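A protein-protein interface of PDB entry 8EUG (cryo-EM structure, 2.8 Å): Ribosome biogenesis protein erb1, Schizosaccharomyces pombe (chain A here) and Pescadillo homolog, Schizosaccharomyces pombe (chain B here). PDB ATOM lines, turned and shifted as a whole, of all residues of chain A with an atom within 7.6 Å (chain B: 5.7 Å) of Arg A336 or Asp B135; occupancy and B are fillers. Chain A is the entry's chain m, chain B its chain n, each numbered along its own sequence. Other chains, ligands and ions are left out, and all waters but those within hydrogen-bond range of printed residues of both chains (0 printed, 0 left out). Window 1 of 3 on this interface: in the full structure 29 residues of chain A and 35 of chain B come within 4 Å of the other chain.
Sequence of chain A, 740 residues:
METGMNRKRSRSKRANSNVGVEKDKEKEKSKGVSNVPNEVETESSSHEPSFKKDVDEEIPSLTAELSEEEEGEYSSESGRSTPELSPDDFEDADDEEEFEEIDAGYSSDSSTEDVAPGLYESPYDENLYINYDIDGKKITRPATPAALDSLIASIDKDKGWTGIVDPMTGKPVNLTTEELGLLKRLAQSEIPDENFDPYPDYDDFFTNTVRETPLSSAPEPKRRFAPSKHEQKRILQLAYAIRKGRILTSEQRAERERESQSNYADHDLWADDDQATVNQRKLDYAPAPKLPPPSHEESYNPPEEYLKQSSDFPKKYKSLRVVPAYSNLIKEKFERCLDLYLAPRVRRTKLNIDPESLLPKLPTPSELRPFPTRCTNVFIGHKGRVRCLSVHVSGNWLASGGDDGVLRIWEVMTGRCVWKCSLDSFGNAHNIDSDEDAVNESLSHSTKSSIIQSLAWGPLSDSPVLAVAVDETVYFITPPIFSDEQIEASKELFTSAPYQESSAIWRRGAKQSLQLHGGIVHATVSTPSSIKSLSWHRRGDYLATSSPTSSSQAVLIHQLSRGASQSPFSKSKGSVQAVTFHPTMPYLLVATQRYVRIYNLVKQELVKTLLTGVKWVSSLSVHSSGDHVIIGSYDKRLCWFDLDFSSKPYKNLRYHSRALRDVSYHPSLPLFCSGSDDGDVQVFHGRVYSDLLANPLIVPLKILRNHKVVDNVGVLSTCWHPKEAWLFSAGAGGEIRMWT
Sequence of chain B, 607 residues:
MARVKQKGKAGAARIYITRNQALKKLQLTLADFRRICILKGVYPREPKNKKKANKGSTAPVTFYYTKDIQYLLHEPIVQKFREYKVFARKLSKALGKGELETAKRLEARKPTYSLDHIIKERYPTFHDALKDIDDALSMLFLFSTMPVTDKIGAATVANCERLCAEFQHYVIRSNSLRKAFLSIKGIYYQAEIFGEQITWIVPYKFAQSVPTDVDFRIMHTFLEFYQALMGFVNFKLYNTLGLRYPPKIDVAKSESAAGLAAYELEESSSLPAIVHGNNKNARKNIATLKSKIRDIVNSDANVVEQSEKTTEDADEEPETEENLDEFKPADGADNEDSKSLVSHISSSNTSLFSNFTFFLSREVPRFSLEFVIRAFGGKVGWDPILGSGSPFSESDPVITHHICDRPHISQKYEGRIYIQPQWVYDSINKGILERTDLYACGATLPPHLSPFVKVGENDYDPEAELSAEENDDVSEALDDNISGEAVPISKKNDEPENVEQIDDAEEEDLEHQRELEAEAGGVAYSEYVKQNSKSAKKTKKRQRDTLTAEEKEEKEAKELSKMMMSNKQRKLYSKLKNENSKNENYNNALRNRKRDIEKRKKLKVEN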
ATOM      1  N   ALA A 288       4.069  25.568  12.772  1.00  0.00           N
ATOM      2  CA  ALA A 288       4.267  25.177  14.158  1.00  0.00           C
ATOM      3  C   ALA A 288       3.354  25.977  15.088  1.00  0.00           C
ATOM      4  O   ALA A 288       3.011  27.128  14.802  1.00  0.00           O
ATOM      5  CB  ALA A 288       5.725  25.377  14.564  1.00  0.00           C
ATOM      6  N   PRO A 289       2.944  25.385  16.210  1.00  0.00           N
ATOM      7  CA  PRO A 289       2.056  26.094  17.142  1.00  0.00           C
ATOM      8  C   PRO A 289       2.769  27.113  18.020  1.00  0.00           C
ATOM      9  O   PRO A 289       2.200  27.542  19.029  1.00  0.00           O
ATOM     10  CB  PRO A 289       1.465  24.959  17.987  1.00  0.00           C
ATOM     11  CG  PRO A 289       2.491  23.883  17.928  1.00  0.00           C
ATOM     12  CD  PRO A 289       3.070  23.957  16.548  1.00  0.00           C
ATOM     13  N   LYS A 290       4.007  27.478  17.673  1.00  0.00           N
ATOM     14  CA  LYS A 290       4.807  28.479  18.392  1.00  0.00           C
ATOM     15  C   LYS A 290       4.815  28.205  19.902  1.00  0.00           C
ATOM     16  O   LYS A 290       4.174  28.879  20.708  1.00  0.00           O
ATOM     17  CB  LYS A 290       4.386  29.918  18.044  1.00  0.00           C
ATOM     18  CG  LYS A 290       2.959  30.351  18.354  1.00  0.00           C
ATOM     19  CD  LYS A 290       2.343  30.995  17.124  1.00  0.00           C
ATOM     20  CE  LYS A 290       1.811  29.958  16.149  1.00  0.00           C
ATOM     21  NZ  LYS A 290       1.503  30.580  14.835  1.00  0.00           N
ATOM     22  N   LEU A 291       5.549  27.140  20.239  1.00  0.00           N
ATOM     23  CA  LEU A 291       5.762  26.599  21.578  1.00  0.00           C
ATOM     24  C   LEU A 291       5.903  27.705  22.618  1.00  0.00           C
ATOM     25  O   LEU A 291       6.572  28.715  22.364  1.00  0.00           O
ATOM     26  CB  LEU A 291       7.013  25.717  21.582  1.00  0.00           C
ATOM     27  CG  LEU A 291       7.031  24.569  20.570  1.00  0.00           C
ATOM     28  CD1 LEU A 291       8.378  23.854  20.567  1.00  0.00           C
ATOM     29  CD2 LEU A 291       5.903  23.593  20.851  1.00  0.00           C
ATOM     30  N   PRO A 292       5.288  27.556  23.791  1.00  0.00           N
ATOM     31  CA  PRO A 292       5.281  28.653  24.752  1.00  0.00           C
ATOM     32  C   PRO A 292       6.678  28.941  25.251  1.00  0.00           C
ATOM     33  O   PRO A 292       7.559  28.059  25.239  1.00  0.00           O
ATOM     34  CB  PRO A 292       4.376  28.131  25.876  1.00  0.00           C
ATOM     35  CG  PRO A 292       4.507  26.658  25.800  1.00  0.00           C
ATOM     36  CD  PRO A 292       4.671  26.335  24.340  1.00  0.00           C
ATOM     37  N   ILE A 330      -3.648  23.156  35.964  1.00  0.00           N
ATOM     38  CA  ILE A 330      -4.648  22.605  35.055  1.00  0.00           C
ATOM     39  C   ILE A 330      -5.240  23.710  34.186  1.00  0.00           C
ATOM     40  O   ILE A 330      -5.554  23.495  33.009  1.00  0.00           O
ATOM     41  CB  ILE A 330      -5.735  21.855  35.847  1.00  0.00           C
ATOM     42  CG1 ILE A 330      -5.115  20.721  36.667  1.00  0.00           C
ATOM     43  CG2 ILE A 330      -6.797  21.299  34.912  1.00  0.00           C
ATOM     44  CD1 ILE A 330      -4.916  21.056  38.131  1.00  0.00           C
ATOM     45  N   LYS A 331      -5.396  24.910  34.750  1.00  0.00           N
ATOM     46  CA  LYS A 331      -6.005  26.008  34.003  1.00  0.00           C
ATOM     47  C   LYS A 331      -5.106  26.484  32.865  1.00  0.00           C
ATOM     48  O   LYS A 331      -5.589  26.710  31.749  1.00  0.00           O
ATOM     49  CB  LYS A 331      -6.339  27.161  34.947  1.00  0.00           C
ATOM     50  CG  LYS A 331      -7.047  28.333  34.290  1.00  0.00           C
ATOM     51  CD  LYS A 331      -8.497  27.999  33.984  1.00  0.00           C
ATOM     52  CE  LYS A 331      -9.269  29.235  33.554  1.00  0.00           C
ATOM     53  NZ  LYS A 331      -8.882  29.691  32.191  1.00  0.00           N
ATOM     54  N   GLU A 332      -3.803  26.657  33.120  1.00  0.00           N
ATOM     55  CA  GLU A 332      -2.908  27.054  32.033  1.00  0.00           C
ATOM     56  C   GLU A 332      -2.818  25.969  30.969  1.00  0.00           C
ATOM     57  O   GLU A 332      -2.789  26.269  29.770  1.00  0.00           O
ATOM     58  CB  GLU A 332      -1.506  27.391  32.549  1.00  0.00           C
ATOM     59  CG  GLU A 332      -1.367  28.747  33.228  1.00  0.00           C
ATOM     60  CD  GLU A 332      -1.590  28.685  34.720  1.00  0.00           C
ATOM     61  OE1 GLU A 332      -1.710  27.565  35.250  1.00  0.00           O
ATOM     62  OE2 GLU A 332      -1.644  29.754  35.363  1.00  0.00           O
ATOM     63  N   LYS A 333      -2.767  24.703  31.388  1.00  0.00           N
ATOM     64  CA  LYS A 333      -2.745  23.608  30.425  1.00  0.00           C
ATOM     65  C   LYS A 333      -4.018  23.576  29.592  1.00  0.00           C
ATOM     66  O   LYS A 333      -3.969  23.319  28.384  1.00  0.00           O
ATOM     67  CB  LYS A 333      -2.542  22.277  31.146  1.00  0.00           C
ATOM     68  CG  LYS A 333      -1.173  22.113  31.767  1.00  0.00           C
ATOM     69  CD  LYS A 333      -0.097  22.216  30.706  1.00  0.00           C
ATOM     70  CE  LYS A 333      -0.249  21.091  29.700  1.00  0.00           C
ATOM     71  NZ  LYS A 333      -0.086  19.766  30.347  1.00  0.00           N
ATOM     72  N   PHE A 334      -5.167  23.824  30.222  1.00  0.00           N
ATOM     73  CA  PHE A 334      -6.410  23.908  29.467  1.00  0.00           C
ATOM     74  C   PHE A 334      -6.392  25.095  28.513  1.00  0.00           C
ATOM     75  O   PHE A 334      -6.885  25.002  27.383  1.00  0.00           O
ATOM     76  CB  PHE A 334      -7.601  23.997  30.420  1.00  0.00           C
ATOM     77  CG  PHE A 334      -8.918  24.128  29.721  1.00  0.00           C
ATOM     78  CD1 PHE A 334      -9.386  23.109  28.908  1.00  0.00           C
ATOM     79  CD2 PHE A 334      -9.689  25.266  29.870  1.00  0.00           C
ATOM     80  CE1 PHE A 334     -10.597  23.222  28.260  1.00  0.00           C
ATOM     81  CE2 PHE A 334     -10.901  25.382  29.224  1.00  0.00           C
ATOM     82  CZ  PHE A 334     -11.357  24.359  28.418  1.00  0.00           C
ATOM     83  N   GLU A 335      -5.831  26.225  28.955  1.00  0.00           N
ATOM     84  CA  GLU A 335      -5.696  27.382  28.076  1.00  0.00           C
ATOM     85  C   GLU A 335      -4.774  27.078  26.903  1.00  0.00           C
ATOM     86  O   GLU A 335      -5.039  27.498  25.770  1.00  0.00           O
ATOM     87  CB  GLU A 335      -5.181  28.585  28.866  1.00  0.00           C
ATOM     88  CG  GLU A 335      -5.002  29.861  28.046  1.00  0.00           C
ATOM     89  CD  GLU A 335      -6.288  30.342  27.397  1.00  0.00           C
ATOM     90  OE1 GLU A 335      -6.607  29.883  26.279  1.00  0.00           O
ATOM     91  OE2 GLU A 335      -6.981  31.186  28.005  1.00  0.00           O
ATOM     92  N   ARG A 336      -3.681  26.355  27.155  1.00  0.00           N
ATOM     93  CA  ARG A 336      -2.801  25.947  26.064  1.00  0.00           C
ATOM     94  C   ARG A 336      -3.531  25.046  25.077  1.00  0.00           C
ATOM     95  O   ARG A 336      -3.395  25.210  23.859  1.00  0.00           O
ATOM     96  CB  ARG A 336      -1.565  25.240  26.619  1.00  0.00           C
ATOM     97  CG  ARG A 336      -0.666  24.653  25.545  1.00  0.00           C
ATOM     98  CD  ARG A 336       0.049  25.735  24.758  1.00  0.00           C
ATOM     99  NE  ARG A 336       1.034  25.171  23.843  1.00  0.00           N
ATOM    100  CZ  ARG A 336       1.379  25.715  22.685  1.00  0.00           C
ATOM    101  NH1 ARG A 336       0.842  26.849  22.267  1.00  0.00           N
ATOM    102  NH2 ARG A 336       2.287  25.106  21.927  1.00  0.00           N
ATOM    103  N   CYS A 337      -4.314  24.092  25.584  1.00  0.00           N
ATOM    104  CA  CYS A 337      -5.083  23.222  24.702  1.00  0.00           C
ATOM    105  C   CYS A 337      -6.100  24.020  23.899  1.00  0.00           C
ATOM    106  O   CYS A 337      -6.357  23.716  22.728  1.00  0.00           O
ATOM    107  CB  CYS A 337      -5.772  22.129  25.517  1.00  0.00           C
ATOM    108  SG  CYS A 337      -4.894  20.553  25.517  1.00  0.00           S
ATOM    109  N   LEU A 338      -6.700  25.040  24.518  1.00  0.00           N
ATOM    110  CA  LEU A 338      -7.613  25.912  23.788  1.00  0.00           C
ATOM    111  C   LEU A 338      -6.888  26.662  22.678  1.00  0.00           C
ATOM    112  O   LEU A 338      -7.414  26.803  21.568  1.00  0.00           O
ATOM    113  CB  LEU A 338      -8.276  26.896  24.748  1.00  0.00           C
ATOM    114  CG  LEU A 338      -9.367  26.342  25.663  1.00  0.00           C
ATOM    115  CD1 LEU A 338     -10.002  27.473  26.445  1.00  0.00           C
ATOM    116  CD2 LEU A 338     -10.412  25.576  24.872  1.00  0.00           C
ATOM    117  N   ASP A 339      -5.677  27.148  22.959  1.00  0.00           N
ATOM    118  CA  ASP A 339      -4.930  27.905  21.961  1.00  0.00           C
ATOM    119  C   ASP A 339      -4.515  27.033  20.784  1.00  0.00           C
ATOM    120  O   ASP A 339      -4.319  27.546  19.677  1.00  0.00           O
ATOM    121  CB  ASP A 339      -3.701  28.548  22.605  1.00  0.00           C
ATOM    122  CG  ASP A 339      -4.044  29.790  23.401  1.00  0.00           C
ATOM    123  OD1 ASP A 339      -5.229  29.960  23.756  1.00  0.00           O
ATOM    124  OD2 ASP A 339      -3.129  30.592  23.678  1.00  0.00           O
ATOM    125  N   LEU A 340      -4.370  25.725  21.002  1.00  0.00           N
ATOM    126  CA  LEU A 340      -3.955  24.829  19.929  1.00  0.00           C
ATOM    127  C   LEU A 340      -5.001  24.708  18.828  1.00  0.00           C
ATOM    128  O   LEU A 340      -4.669  24.266  17.724  1.00  0.00           O
ATOM    129  CB  LEU A 340      -3.635  23.446  20.497  1.00  0.00           C
ATOM    130  CG  LEU A 340      -2.400  23.354  21.395  1.00  0.00           C
ATOM    131  CD1 LEU A 340      -2.263  21.958  21.981  1.00  0.00           C
ATOM    132  CD2 LEU A 340      -1.145  23.746  20.632  1.00  0.00           C
ATOM    133  N   TYR A 341      -6.253  25.082  19.098  1.00  0.00           N
ATOM    134  CA  TYR A 341      -7.297  24.975  18.089  1.00  0.00           C
ATOM    135  C   TYR A 341      -8.208  26.192  18.002  1.00  0.00           C
ATOM    136  O   TYR A 341      -9.081  26.218  17.129  1.00  0.00           O
ATOM    137  CB  TYR A 341      -8.153  23.723  18.340  1.00  0.00           C
ATOM    138  CG  TYR A 341      -9.221  23.902  19.395  1.00  0.00           C
ATOM    139  CD1 TYR A 341      -8.897  23.918  20.745  1.00  0.00           C
ATOM    140  CD2 TYR A 341     -10.557  24.036  19.042  1.00  0.00           C
ATOM    141  CE1 TYR A 341      -9.871  24.072  21.710  1.00  0.00           C
ATOM    142  CE2 TYR A 341     -11.536  24.193  20.001  1.00  0.00           C
ATOM    143  CZ  TYR A 341     -11.188  24.209  21.334  1.00  0.00           C
ATOM    144  OH  TYR A 341     -12.161  24.365  22.294  1.00  0.00           O
ATOM    145  N   LEU A 342      -8.040  27.193  18.862  1.00  0.00           N
ATOM    146  CA  LEU A 342      -8.826  28.416  18.784  1.00  0.00           C
ATOM    147  C   LEU A 342      -8.008  29.637  18.401  1.00  0.00           C
ATOM    148  O   LEU A 342      -8.514  30.504  17.688  1.00  0.00           O
ATOM    149  CB  LEU A 342      -9.526  28.691  20.121  1.00  0.00           C
ATOM    150  CG  LEU A 342     -10.747  27.831  20.451  1.00  0.00           C
ATOM    151  CD1 LEU A 342     -11.426  28.333  21.715  1.00  0.00           C
ATOM    152  CD2 LEU A 342     -11.722  27.814  19.286  1.00  0.00           C
ATOM    153  N   ALA A 343      -6.765  29.723  18.856  1.00  0.00           N
ATOM    154  CA  ALA A 343      -5.905  30.836  18.482  1.00  0.00           C
ATOM    155  C   ALA A 343      -5.390  30.636  17.061  1.00  0.00           C
ATOM    156  O   ALA A 343      -4.801  29.592  16.764  1.00  0.00           O
ATOM    157  CB  ALA A 343      -4.732  30.962  19.449  1.00  0.00           C
ATOM    158  N   ARG A 345      -2.976  30.634  13.912  1.00  0.00           N
ATOM    159  CA  ARG A 345      -1.535  30.449  13.819  1.00  0.00           C
ATOM    160  C   ARG A 345      -1.000  31.214  12.617  1.00  0.00           C
ATOM    161  O   ARG A 345      -1.444  30.990  11.484  1.00  0.00           O
ATOM    162  CB  ARG A 345      -1.171  28.967  13.720  1.00  0.00           C
ATOM    163  CG  ARG A 345      -1.508  28.167  14.965  1.00  0.00           C
ATOM    164  CD  ARG A 345      -1.168  26.699  14.790  1.00  0.00           C
ATOM    165  NE  ARG A 345      -2.060  25.838  15.556  1.00  0.00           N
ATOM    166  CZ  ARG A 345      -2.117  24.519  15.431  1.00  0.00           C
ATOM    167  NH1 ARG A 345      -1.341  23.872  14.577  1.00  0.00           N
ATOM    168  NH2 ARG A 345      -2.974  23.832  16.180  1.00  0.00           N
ATOM    169  N   ASP B 132       6.574  17.907  17.625  1.00  0.00           N
ATOM    170  CA  ASP B 132       5.292  18.222  18.256  1.00  0.00           C
ATOM    171  C   ASP B 132       4.889  17.095  19.208  1.00  0.00           C
ATOM    172  O   ASP B 132       3.916  16.372  18.995  1.00  0.00           O
ATOM    173  CB  ASP B 132       4.225  18.464  17.192  1.00  0.00           C
ATOM    174  CG  ASP B 132       2.969  19.096  17.760  1.00  0.00           C
ATOM    175  OD1 ASP B 132       3.005  20.300  18.092  1.00  0.00           O
ATOM    176  OD2 ASP B 132       1.946  18.390  17.876  1.00  0.00           O
ATOM    177  N   ILE B 133       5.664  16.957  20.280  1.00  0.00           N
ATOM    178  CA  ILE B 133       5.409  15.902  21.255  1.00  0.00           C
ATOM    179  C   ILE B 133       5.405  16.471  22.667  1.00  0.00           C
ATOM    180  O   ILE B 133       4.948  15.814  23.609  1.00  0.00           O
ATOM    181  CB  ILE B 133       6.442  14.770  21.124  1.00  0.00           C
ATOM    182  CG1 ILE B 133       5.833  13.442  21.572  1.00  0.00           C
ATOM    183  CG2 ILE B 133       7.680  15.082  21.946  1.00  0.00           C
ATOM    184  CD1 ILE B 133       6.669  12.238  21.206  1.00  0.00           C
ATOM    185  N   ASP B 134       5.913  17.696  22.826  1.00  0.00           N
ATOM    186  CA  ASP B 134       6.046  18.269  24.162  1.00  0.00           C
ATOM    187  C   ASP B 134       4.686  18.514  24.804  1.00  0.00           C
ATOM    188  O   ASP B 134       4.515  18.298  26.009  1.00  0.00           O
ATOM    189  CB  ASP B 134       6.859  19.561  24.104  1.00  0.00           C
ATOM    190  CG  ASP B 134       6.209  20.624  23.244  1.00  0.00           C
ATOM    191  OD1 ASP B 134       5.377  20.268  22.383  1.00  0.00           O
ATOM    192  OD2 ASP B 134       6.526  21.816  23.436  1.00  0.00           O
ATOM    193  N   ASP B 135       3.710  18.978  24.020  1.00  0.00           N
ATOM    194  CA  ASP B 135       2.371  19.191  24.560  1.00  0.00           C
ATOM    195  C   ASP B 135       1.721  17.873  24.961  1.00  0.00           C
ATOM    196  O   ASP B 135       1.020  17.804  25.978  1.00  0.00           O
ATOM    197  CB  ASP B 135       1.512  19.942  23.545  1.00  0.00           C
ATOM    198  CG  ASP B 135       1.880  21.409  23.448  1.00  0.00           C
ATOM    199  OD1 ASP B 135       2.586  21.899  24.355  1.00  0.00           O
ATOM    200  OD2 ASP B 135       1.471  22.073  22.472  1.00  0.00           O
ATOM    201  N   ALA B 136       1.935  16.820  24.170  1.00  0.00           N
ATOM    202  CA  ALA B 136       1.423  15.502  24.528  1.00  0.00           C
ATOM    203  C   ALA B 136       2.038  15.008  25.831  1.00  0.00           C
ATOM    204  O   ALA B 136       1.341  14.465  26.695  1.00  0.00           O
ATOM    205  CB  ALA B 136       1.692  14.508  23.398  1.00  0.00           C
ATOM    206  N   LEU B 137       3.352  15.187  25.987  1.00  0.00           N
ATOM    207  CA  LEU B 137       4.011  14.763  27.219  1.00  0.00           C
ATOM    208  C   LEU B 137       3.466  15.517  28.422  1.00  0.00           C
ATOM    209  O   LEU B 137       3.200  14.920  29.471  1.00  0.00           O
ATOM    210  CB  LEU B 137       5.520  14.978  27.114  1.00  0.00           C
ATOM    211  CG  LEU B 137       6.333  14.222  26.067  1.00  0.00           C
ATOM    212  CD1 LEU B 137       7.695  13.928  26.641  1.00  0.00           C
ATOM    213  CD2 LEU B 137       5.656  12.935  25.663  1.00  0.00           C
ATOM    214  N   SER B 138       3.294  16.832  28.286  1.00  0.00           N
ATOM    215  CA  SER B 138       2.800  17.633  29.400  1.00  0.00           C
ATOM    216  C   SER B 138       1.403  17.190  29.815  1.00  0.00           C
ATOM    217  O   SER B 138       1.091  17.124  31.008  1.00  0.00           O
ATOM    218  CB  SER B 138       2.812  19.116  29.026  1.00  0.00           C
ATOM    219  OG  SER B 138       4.120  19.555  28.707  1.00  0.00           O
ATOM    220  N   MET B 139       0.540  16.900  28.839  1.00  0.00           N
ATOM    221  CA  MET B 139      -0.820  16.482  29.164  1.00  0.00           C
ATOM    222  C   MET B 139      -0.837  15.108  29.825  1.00  0.00           C
ATOM    223  O   MET B 139      -1.546  14.897  30.816  1.00  0.00           O
ATOM    224  CB  MET B 139      -1.686  16.487  27.903  1.00  0.00           C
ATOM    225  CG  MET B 139      -3.178  16.333  28.164  1.00  0.00           C
ATOM    226  SD  MET B 139      -4.035  17.876  28.560  1.00  0.00           S
ATOM    227  CE  MET B 139      -2.838  19.112  28.057  1.00  0.00           C
ATOM    228  N   LEU B 140      -0.066  14.159  29.286  1.00  0.00           N
ATOM    229  CA  LEU B 140      -0.042  12.814  29.855  1.00  0.00           C
ATOM    230  C   LEU B 140       0.511  12.819  31.274  1.00  0.00           C
ATOM    231  O   LEU B 140      -0.048  12.170  32.168  1.00  0.00           O
ATOM    232  CB  LEU B 140       0.780  11.880  28.970  1.00  0.00           C
ATOM    233  CG  LEU B 140       0.220  11.546  27.588  1.00  0.00           C
ATOM    234  CD1 LEU B 140       1.159  10.602  26.860  1.00  0.00           C
ATOM    235  CD2 LEU B 140      -1.168  10.939  27.707  1.00  0.00           C
ATOM    236  N   THR B 199      10.694  19.618  25.955  1.00  0.00           N
ATOM    237  CA  THR B 199      10.526  20.118  27.312  1.00  0.00           C
ATOM    238  C   THR B 199       9.111  19.813  27.783  1.00  0.00           C
ATOM    239  O   THR B 199       8.148  19.991  27.030  1.00  0.00           O
ATOM    240  CB  THR B 199      10.826  21.622  27.394  1.00  0.00           C
ATOM    241  OG1 THR B 199      10.727  22.062  28.755  1.00  0.00           O
ATOM    242  CG2 THR B 199       9.877  22.430  26.516  1.00  0.00           C
ATOM    243  N   TYR B 226      -3.356  12.263  21.833  1.00  0.00           N
ATOM    244  CA  TYR B 226      -1.995  12.135  22.341  1.00  0.00           C
ATOM    245  C   TYR B 226      -1.648  10.683  22.645  1.00  0.00           C
ATOM    246  O   TYR B 226      -0.528  10.241  22.372  1.00  0.00           O
ATOM    247  CB  TYR B 226      -1.810  12.999  23.586  1.00  0.00           C
ATOM    248  CG  TYR B 226      -1.835  14.482  23.306  1.00  0.00           C
ATOM    249  CD1 TYR B 226      -1.511  14.979  22.051  1.00  0.00           C
ATOM    250  CD2 TYR B 226      -2.178  15.387  24.301  1.00  0.00           C
ATOM    251  CE1 TYR B 226      -1.532  16.335  21.794  1.00  0.00           C
ATOM    252  CE2 TYR B 226      -2.202  16.742  24.054  1.00  0.00           C
ATOM    253  CZ  TYR B 226      -1.880  17.211  22.800  1.00  0.00           C
ATOM    254  OH  TYR B 226      -1.904  18.565  22.554  1.00  0.00           O
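The side-chain amino group (NZ) of Lys A333 is in hydrogen-bond range of the backbone carbonyl oxygen (O) of Ser B138, at 3.0 Å.
NH2 of Arg A336 lies within salt-bridge range of OD2 of Asp B135, 3.2 Å away.
NZ of Lys A333 lies close to N of Met B139 (3.3 Å).
Of the 20 printed residues of chain A, 6 touch a printed residue of chain B.
Along chain B the printed residues that touch a printed residue of chain A span positions 132 to 226.
Among the printed residues, 8 pairs touch across the chains.
Among the printed residues, Asp or Glu carboxylates within 4 Å of a Lys or Arg side-chain nitrogen of the other chain: Arg A336 with Asp B135 (3.2 Å).
Arg A336 touches one residue of chain B.
Asp B135 touches just these residues of chain A: Arg A336 and Leu A340.
Of the printed residues of chain B, Cys A337 touches Met B139 (3.6 Å).
Of the printed residues of chain B, Lys A333 touches Ser B138 and Met B139.
Of the printed residues of chain B, Leu A340 touches Asp B135 (3.6 Å) and Tyr B226 (3.5 Å).
Of the printed residues of chain A, Met B139 touches Lys A333 (3.3 Å) and Cys A337 (3.6 Å).
The nearest residue of chain B that does not touch Arg A336 is Asp B134 (5.6 Å).
The nearest printed residue of chain A that does not touch Asp B135 is Pro A292 (4.9 Å).
The nearest printed residue of chain B that does not touch Pro A289 is Asp B135 (5.0 Å).
CG of Pro A289 touches OD1 of Asp B132, at 3.6 Å.
Leu A291 touches Asp B134 (CD2 to OD2, 3.2 Å).
Met B139 touches Cys A337 (CE to SG, 3.6 Å).
CD2 of Leu A340 touches OD2 of Asp B135, at 3.6 Å.
Leu A340 touches Tyr B226.
OG of Ser B138 is in hydrogen-bond range of O of Asp B134.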
